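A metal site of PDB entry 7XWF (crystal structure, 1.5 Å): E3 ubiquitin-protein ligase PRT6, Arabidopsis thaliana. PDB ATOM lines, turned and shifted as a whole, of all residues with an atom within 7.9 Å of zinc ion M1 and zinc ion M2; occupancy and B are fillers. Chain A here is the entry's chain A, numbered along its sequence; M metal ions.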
ATOM      1  N   GLY A   7       6.912 -17.366  23.840  1.00  0.00           N
ATOM      2  CA  GLY A   7       6.972 -16.107  23.132  1.00  0.00           C
ATOM      3  C   GLY A   7       6.684 -14.892  23.995  1.00  0.00           C
ATOM      4  O   GLY A   7       5.603 -14.767  24.574  1.00  0.00           O
ATOM      5  N   VAL A   8       7.664 -13.992  24.103  1.00  0.00           N
ATOM      6  CA  VAL A   8       7.470 -12.669  24.680  1.00  0.00           C
ATOM      7  C   VAL A   8       7.121 -11.732  23.539  1.00  0.00           C
ATOM      8  O   VAL A   8       7.649 -11.861  22.436  1.00  0.00           O
ATOM      9  CB  VAL A   8       8.755 -12.209  25.396  1.00  0.00           C
ATOM     10  CG1 VAL A   8       8.631 -10.757  25.826  1.00  0.00           C
ATOM     11  CG2 VAL A   8       9.055 -13.103  26.576  1.00  0.00           C
ATOM     12  N   CYS A   9       6.245 -10.762  23.804  1.00  0.00           N
ATOM     13  CA  CYS A   9       5.871  -9.805  22.767  1.00  0.00           C
ATOM     14  C   CYS A   9       7.095  -9.015  22.307  1.00  0.00           C
ATOM     15  O   CYS A   9       7.403  -8.959  21.113  1.00  0.00           O
ATOM     16  CB  CYS A   9       4.795  -8.845  23.288  1.00  0.00           C
ATOM     17  SG  CYS A   9       4.305  -7.535  22.122  1.00  0.00           S
ATOM     18  N   GLY A  10       7.752  -8.339  23.237  1.00  0.00           N
ATOM     19  CA  GLY A  10       8.934  -7.559  22.950  1.00  0.00           C
ATOM     20  C   GLY A  10       8.790  -6.352  22.043  1.00  0.00           C
ATOM     21  O   GLY A  10       9.816  -5.726  21.710  1.00  0.00           O
ATOM     22  N   SER A  11       7.565  -5.989  21.641  1.00  0.00           N
ATOM     23  CA  SER A  11       7.362  -4.848  20.760  1.00  0.00           C
ATOM     24  C   SER A  11       7.945  -3.596  21.394  1.00  0.00           C
ATOM     25  O   SER A  11       7.809  -3.382  22.602  1.00  0.00           O
ATOM     26  CB  SER A  11       5.866  -4.618  20.550  1.00  0.00           C
ATOM     27  OG  SER A  11       5.322  -5.595  19.672  1.00  0.00           O
ATOM     28  N   VAL A  12       8.536  -2.727  20.576  1.00  0.00           N
ATOM     29  CA  VAL A  12       9.369  -1.632  21.057  1.00  0.00           C
ATOM     30  C   VAL A  12       8.688  -0.294  20.862  1.00  0.00           C
ATOM     31  O   VAL A  12       8.098  -0.031  19.810  1.00  0.00           O
ATOM     32  CB  VAL A  12      10.763  -1.661  20.397  1.00  0.00           C
ATOM     33  CG1 VAL A  12      11.581  -0.432  20.806  1.00  0.00           C
ATOM     34  CG2 VAL A  12      11.483  -2.947  20.720  1.00  0.00           C
ATOM     35  N   TRP A  13       8.797   0.571  21.870  1.00  0.00           N
ATOM     36  CA  TRP A  13       8.223   1.904  21.832  1.00  0.00           C
ATOM     37  C   TRP A  13       9.306   2.937  21.605  1.00  0.00           C
ATOM     38  O   TRP A  13      10.428   2.784  22.089  1.00  0.00           O
ATOM     39  CB  TRP A  13       7.531   2.279  23.153  1.00  0.00           C
ATOM     40  CG  TRP A  13       6.503   1.341  23.529  1.00  0.00           C
ATOM     41  CD1 TRP A  13       5.409   1.024  22.818  1.00  0.00           C
ATOM     42  CD2 TRP A  13       6.476   0.536  24.700  1.00  0.00           C
ATOM     43  NE1 TRP A  13       4.680   0.075  23.460  1.00  0.00           N
ATOM     44  CE2 TRP A  13       5.312  -0.253  24.628  1.00  0.00           C
ATOM     45  CE3 TRP A  13       7.307   0.405  25.820  1.00  0.00           C
ATOM     46  CZ2 TRP A  13       4.948  -1.154  25.613  1.00  0.00           C
ATOM     47  CZ3 TRP A  13       6.948  -0.509  26.807  1.00  0.00           C
ATOM     48  CH2 TRP A  13       5.769  -1.266  26.699  1.00  0.00           C
ATOM     49  N   ALA A  32       5.267  -2.528  31.606  1.00  0.00           N
ATOM     50  CA  ALA A  32       4.190  -1.994  30.784  1.00  0.00           C
ATOM     51  C   ALA A  32       3.881  -2.968  29.661  1.00  0.00           C
ATOM     52  O   ALA A  32       4.718  -3.799  29.286  1.00  0.00           O
ATOM     53  CB  ALA A  32       4.541  -0.641  30.168  1.00  0.00           C
ATOM     54  N   ILE A  33       2.697  -2.833  29.077  1.00  0.00           N
ATOM     55  CA  ILE A  33       2.368  -3.629  27.909  1.00  0.00           C
ATOM     56  C   ILE A  33       1.823  -2.736  26.799  1.00  0.00           C
ATOM     57  O   ILE A  33       1.235  -1.682  27.043  1.00  0.00           O
ATOM     58  CB  ILE A  33       1.434  -4.811  28.173  1.00  0.00           C
ATOM     59  CG1 ILE A  33       0.120  -4.349  28.766  1.00  0.00           C
ATOM     60  CG2 ILE A  33       2.156  -5.817  29.081  1.00  0.00           C
ATOM     61  CD1 ILE A  33      -0.902  -5.493  28.875  1.00  0.00           C
ATOM     62  N   CYS A  34       2.007  -3.205  25.581  1.00  0.00           N
ATOM     63  CA  CYS A  34       1.585  -2.463  24.407  1.00  0.00           C
ATOM     64  C   CYS A  34       0.062  -2.449  24.291  1.00  0.00           C
ATOM     65  O   CYS A  34      -0.650  -3.290  24.861  1.00  0.00           O
ATOM     66  CB  CYS A  34       2.268  -3.020  23.160  1.00  0.00           C
ATOM     67  SG  CYS A  34       1.662  -4.611  22.559  1.00  0.00           S
ATOM     68  N   VAL A  35      -0.448  -1.467  23.548  1.00  0.00           N
ATOM     69  CA  VAL A  35      -1.896  -1.348  23.413  1.00  0.00           C
ATOM     70  C   VAL A  35      -2.529  -2.623  22.876  1.00  0.00           C
ATOM     71  O   VAL A  35      -3.539  -3.074  23.440  1.00  0.00           O
ATOM     72  CB  VAL A  35      -2.244  -0.079  22.601  1.00  0.00           C
ATOM     73  CG1 VAL A  35      -3.738  -0.049  22.332  1.00  0.00           C
ATOM     74  CG2 VAL A  35      -1.796   1.170  23.332  1.00  0.00           C
ATOM     75  N   PRO A  36      -2.036  -3.224  21.790  1.00  0.00           N
ATOM     76  CA  PRO A  36      -2.677  -4.471  21.320  1.00  0.00           C
ATOM     77  C   PRO A  36      -2.694  -5.585  22.354  1.00  0.00           C
ATOM     78  O   PRO A  36      -3.712  -6.283  22.485  1.00  0.00           O
ATOM     79  CB  PRO A  36      -1.847  -4.856  20.085  1.00  0.00           C
ATOM     80  CG  PRO A  36      -1.144  -3.601  19.668  1.00  0.00           C
ATOM     81  CD  PRO A  36      -0.973  -2.757  20.885  1.00  0.00           C
ATOM     82  N   CYS A  37      -1.609  -5.747  23.106  1.00  0.00           N
ATOM     83  CA  CYS A  37      -1.577  -6.765  24.158  1.00  0.00           C
ATOM     84  C   CYS A  37      -2.579  -6.427  25.258  1.00  0.00           C
ATOM     85  O   CYS A  37      -3.286  -7.315  25.751  1.00  0.00           O
ATOM     86  CB  CYS A  37      -0.172  -6.916  24.717  1.00  0.00           C
ATOM     87  SG  CYS A  37       0.954  -7.829  23.610  1.00  0.00           S
ATOM     88  N   PHE A  38      -2.699  -5.151  25.631  1.00  0.00           N
ATOM     89  CA  PHE A  38      -3.727  -4.765  26.576  1.00  0.00           C
ATOM     90  C   PHE A  38      -5.122  -5.142  26.085  1.00  0.00           C
ATOM     91  O   PHE A  38      -5.930  -5.695  26.829  1.00  0.00           O
ATOM     92  CB  PHE A  38      -3.645  -3.278  26.883  1.00  0.00           C
ATOM     93  CG  PHE A  38      -4.638  -2.836  27.912  1.00  0.00           C
ATOM     94  CD1 PHE A  38      -4.340  -2.957  29.263  1.00  0.00           C
ATOM     95  CD2 PHE A  38      -5.882  -2.316  27.549  1.00  0.00           C
ATOM     96  CE1 PHE A  38      -5.256  -2.552  30.223  1.00  0.00           C
ATOM     97  CE2 PHE A  38      -6.792  -1.924  28.512  1.00  0.00           C
ATOM     98  CZ  PHE A  38      -6.477  -2.036  29.840  1.00  0.00           C
ATOM     99  N   ASN A  40      -6.102  -7.377  23.964  1.00  0.00           N
ATOM    100  CA  ASN A  40      -6.354  -8.800  23.804  1.00  0.00           C
ATOM    101  C   ASN A  40      -6.171  -9.576  25.100  1.00  0.00           C
ATOM    102  O   ASN A  40      -6.064 -10.804  25.071  1.00  0.00           O
ATOM    103  CB  ASN A  40      -5.474  -9.345  22.699  1.00  0.00           C
ATOM    104  CG  ASN A  40      -5.896  -8.841  21.336  1.00  0.00           C
ATOM    105  OD1 ASN A  40      -7.080  -8.811  21.012  1.00  0.00           O
ATOM    106  ND2 ASN A  40      -4.917  -8.446  20.544  1.00  0.00           N
ATOM    107  N   GLY A  41      -6.179  -8.885  26.242  1.00  0.00           N
ATOM    108  CA  GLY A  41      -6.177  -9.534  27.534  1.00  0.00           C
ATOM    109  C   GLY A  41      -7.350  -9.046  28.366  1.00  0.00           C
ATOM    110  O   GLY A  41      -8.199  -8.286  27.888  1.00  0.00           O
ATOM    111  N   CYS A  57      10.049  -1.682  25.970  1.00  0.00           N
ATOM    112  CA  CYS A  57       9.518  -2.827  25.265  1.00  0.00           C
ATOM    113  C   CYS A  57       8.408  -3.484  26.071  1.00  0.00           C
ATOM    114  O   CYS A  57       8.384  -3.437  27.303  1.00  0.00           O
ATOM    115  CB  CYS A  57      10.592  -3.849  24.852  1.00  0.00           C
ATOM    116  SG  CYS A  57      11.512  -4.685  26.151  1.00  0.00           S
ATOM    117  N   CYS A  58       7.504  -4.139  25.344  1.00  0.00           N
ATOM    118  CA  CYS A  58       6.330  -4.740  25.962  1.00  0.00           C
ATOM    119  C   CYS A  58       6.722  -5.985  26.764  1.00  0.00           C
ATOM    120  O   CYS A  58       7.473  -6.854  26.307  1.00  0.00           O
ATOM    121  CB  CYS A  58       5.313  -5.156  24.907  1.00  0.00           C
ATOM    122  SG  CYS A  58       3.833  -5.944  25.430  1.00  0.00           S
ATOM    123  N   ASP A  59       6.102  -6.099  27.929  1.00  0.00           N
ATOM    124  CA  ASP A  59       6.399  -7.173  28.872  1.00  0.00           C
ATOM    125  C   ASP A  59       5.421  -8.342  28.785  1.00  0.00           C
ATOM    126  O   ASP A  59       5.584  -9.324  29.509  1.00  0.00           O
ATOM    127  CB  ASP A  59       6.355  -6.600  30.291  1.00  0.00           C
ATOM    128  CG  ASP A  59       7.504  -5.644  30.573  1.00  0.00           C
ATOM    129  OD1 ASP A  59       8.657  -5.999  30.233  1.00  0.00           O
ATOM    130  OD2 ASP A  59       7.268  -4.566  31.149  1.00  0.00           O
ATOM    131  N   CYS A  60       4.429  -8.241  27.897  1.00  0.00           N
ATOM    132  CA  CYS A  60       3.420  -9.282  27.775  1.00  0.00           C
ATOM    133  C   CYS A  60       4.075 -10.603  27.365  1.00  0.00           C
ATOM    134  O   CYS A  60       4.838 -10.656  26.406  1.00  0.00           O
ATOM    135  CB  CYS A  60       2.376  -8.883  26.743  1.00  0.00           C
ATOM    136  SG  CYS A  60       1.021 -10.056  26.643  1.00  0.00           S
ATOM    137  N   GLY A  61       3.797 -11.665  28.133  1.00  0.00           N
ATOM    138  CA  GLY A  61       4.385 -12.960  27.890  1.00  0.00           C
ATOM    139  C   GLY A  61       5.625 -13.257  28.697  1.00  0.00           C
ATOM    140  O   GLY A  61       6.074 -14.416  28.731  1.00  0.00           O
ATOM    141  N   ASP A  62       6.191 -12.254  29.368  1.00  0.00           N
ATOM    142  CA  ASP A  62       7.387 -12.413  30.211  1.00  0.00           C
ATOM    143  C   ASP A  62       6.947 -12.459  31.664  1.00  0.00           C
ATOM    144  O   ASP A  62       6.701 -11.429  32.286  1.00  0.00           O
ATOM    145  CB  ASP A  62       8.323 -11.233  29.969  1.00  0.00           C
ATOM    146  CG  ASP A  62       9.588 -11.296  30.801  1.00  0.00           C
ATOM    147  OD1 ASP A  62       9.761 -12.270  31.574  1.00  0.00           O
ATOM    148  OD2 ASP A  62      10.431 -10.377  30.682  1.00  0.00           O
ATOM    149  N   TRP A  66       5.614  -9.498  34.237  1.00  0.00           N
ATOM    150  CA  TRP A  66       4.175  -9.342  34.146  1.00  0.00           C
ATOM    151  C   TRP A  66       3.505 -10.613  34.640  1.00  0.00           C
ATOM    152  O   TRP A  66       3.951 -11.727  34.317  1.00  0.00           O
ATOM    153  CB  TRP A  66       3.802  -9.046  32.704  1.00  0.00           C
ATOM    154  CG  TRP A  66       2.498  -8.390  32.463  1.00  0.00           C
ATOM    155  CD1 TRP A  66       1.345  -8.980  32.039  1.00  0.00           C
ATOM    156  CD2 TRP A  66       2.222  -6.979  32.542  1.00  0.00           C
ATOM    157  NE1 TRP A  66       0.350  -8.035  31.893  1.00  0.00           N
ATOM    158  CE2 TRP A  66       0.868  -6.796  32.202  1.00  0.00           C
ATOM    159  CE3 TRP A  66       2.986  -5.861  32.900  1.00  0.00           C
ATOM    160  CZ2 TRP A  66       0.270  -5.537  32.164  1.00  0.00           C
ATOM    161  CZ3 TRP A  66       2.376  -4.621  32.901  1.00  0.00           C
ATOM    162  CH2 TRP A  66       1.034  -4.471  32.540  1.00  0.00           C
ATOM    163  N   GLY A  70      -2.347 -11.650  33.368  1.00  0.00           N
ATOM    164  CA  GLY A  70      -2.400 -10.444  32.565  1.00  0.00           C
ATOM    165  C   GLY A  70      -1.847 -10.564  31.171  1.00  0.00           C
ATOM    166  O   GLY A  70      -1.779  -9.536  30.468  1.00  0.00           O
ATOM    167  N   PHE A  71      -1.468 -11.764  30.734  1.00  0.00           N
ATOM    168  CA  PHE A  71      -1.011 -11.965  29.368  1.00  0.00           C
ATOM    169  C   PHE A  71      -2.198 -11.920  28.420  1.00  0.00           C
ATOM    170  O   PHE A  71      -3.327 -12.264  28.770  1.00  0.00           O
ATOM    171  CB  PHE A  71      -0.386 -13.365  29.220  1.00  0.00           C
ATOM    172  CG  PHE A  71       0.933 -13.549  29.928  1.00  0.00           C
ATOM    173  CD1 PHE A  71       1.526 -14.799  29.949  1.00  0.00           C
ATOM    174  CD2 PHE A  71       1.584 -12.494  30.569  1.00  0.00           C
ATOM    175  CE1 PHE A  71       2.735 -15.014  30.587  1.00  0.00           C
ATOM    176  CE2 PHE A  71       2.800 -12.700  31.198  1.00  0.00           C
ATOM    177  CZ  PHE A  71       3.384 -13.957  31.206  1.00  0.00           C
ATOM    178  N   CYS A  72      -1.938 -11.482  27.203  1.00  0.00           N
ATOM    179  CA  CYS A  72      -2.950 -11.510  26.161  1.00  0.00           C
ATOM    180  C   CYS A  72      -3.036 -12.893  25.522  1.00  0.00           C
ATOM    181  O   CYS A  72      -2.213 -13.775  25.779  1.00  0.00           O
ATOM    182  CB  CYS A  72      -2.655 -10.446  25.090  1.00  0.00           C
ATOM    183  SG  CYS A  72      -1.421 -10.924  23.839  1.00  0.00           S
ATOM    184  N   SER A  73      -4.022 -13.044  24.650  1.00  0.00           N
ATOM    185  CA  SER A  73      -4.293 -14.343  24.030  1.00  0.00           C
ATOM    186  C   SER A  73      -3.188 -14.811  23.098  1.00  0.00           C
ATOM    187  O   SER A  73      -3.138 -16.012  22.779  1.00  0.00           O
ATOM    188  CB  SER A  73      -5.600 -14.301  23.259  1.00  0.00           C
ATOM    189  OG  SER A  73      -5.601 -13.269  22.278  1.00  0.00           O
ATOM    190  N   ASN A  74      -2.299 -13.937  22.665  1.00  0.00           N
ATOM    191  CA  ASN A  74      -1.254 -14.336  21.731  1.00  0.00           C
ATOM    192  C   ASN A  74       0.066 -14.662  22.402  1.00  0.00           C
ATOM    193  O   ASN A  74       0.971 -15.165  21.723  1.00  0.00           O
ATOM    194  CB  ASN A  74      -1.040 -13.230  20.683  1.00  0.00           C
ATOM    195  CG  ASN A  74      -2.272 -12.981  19.857  1.00  0.00           C
ATOM    196  OD1 ASN A  74      -2.922 -13.915  19.371  1.00  0.00           O
ATOM    197  ND2 ASN A  74      -2.607 -11.721  19.684  1.00  0.00           N
ATOM    198  N   HIS A  75       0.204 -14.444  23.713  1.00  0.00           N
ATOM    199  CA  HIS A  75       1.482 -14.613  24.394  1.00  0.00           C
ATOM    200  C   HIS A  75       1.379 -15.520  25.599  1.00  0.00           C
ATOM    201  O   HIS A  75       2.071 -15.320  26.608  1.00  0.00           O
ATOM    202  CB  HIS A  75       2.097 -13.260  24.755  1.00  0.00           C
ATOM    203  CG  HIS A  75       2.407 -12.439  23.547  1.00  0.00           C
ATOM    204  ND1 HIS A  75       1.774 -11.252  23.284  1.00  0.00           N
ATOM    205  CD2 HIS A  75       3.221 -12.679  22.499  1.00  0.00           C
ATOM    206  CE1 HIS A  75       2.193 -10.773  22.129  1.00  0.00           C
ATOM    207  NE2 HIS A  75       3.086 -11.624  21.631  1.00  0.00           N
ATOM    208  N   LYS A  76       0.537 -16.544  25.522  1.00  0.00           N
ATOM    209  CA  LYS A  76       0.546 -17.530  26.588  1.00  0.00           C
ATOM    210  C   LYS A  76       0.774 -18.955  26.085  1.00  0.00           C
ATOM    211  O   LYS A  76       1.117 -19.840  26.874  1.00  0.00           O
ATOM    212  CB  LYS A  76      -0.689 -17.495  27.469  1.00  0.00           C
ATOM    213  CG  LYS A  76      -1.921 -16.806  26.964  1.00  0.00           C
ATOM    214  CD  LYS A  76      -2.914 -16.698  28.105  1.00  0.00           C
ATOM    215  CE  LYS A  76      -4.099 -15.867  27.767  1.00  0.00           C
ATOM    216  NZ  LYS A  76      -5.081 -15.791  28.850  1.00  0.00           N
HETATM  217 ZN    ZN M   1       0.632 -10.052  24.446  1.00  0.00          ZN
HETATM  218 ZN    ZN M   2       2.808  -6.397  23.457  1.00  0.00          ZN
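N of Cys 60 lies close to SG of Cys 58 (3.4 Å).
The backbone carbonyl oxygen (O) of Cys 60 lies within hydrogen-bond range of the backbone NH (N) of Cys 9.
The backbone NH of Cys 58 is in hydrogen-bond range of the backbone carbonyl oxygen of Ser 11, 2.9 Å away.
The backbone carbonyl oxygen (O) of Cys 58 sits at hydrogen-bond distance from the backbone NH (N) of Gly 10.
SG of Cys 9 lies close to OG of Ser 11.
The side-chain sulfur (SG) of Cys 72 sits close to the backbone NH (N) of Asn 74, at 3.4 Å.
Within 4 Å of zinc ion M1: Cys 37, Cys 60, Cys 72 and His 75.
Four residues have an atom within 4 Å of zinc ion M2: Cys 9, Cys 34, Cys 37 and Cys 58.
The nearest printed residue that does not touch zinc ion M2 is Cys 60 (4.1 Å).
Zinc ion M1 is bound by ND1 of His 75.
Zinc ion M1 is bound by the side-chain sulfur (SG) of Cys 60 (2.2 Å).
SG of Cys 72 binds zinc ion M1 (2.3 Å).
SG of Cys 37 binds zinc ion M1 (2.4 Å).
Zinc ion M2 is bound by the side-chain sulfur of Cys 58, the side-chain sulfur of Cys 34, the side-chain sulfur of Cys 9 and the side-chain sulfur of Cys 37.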
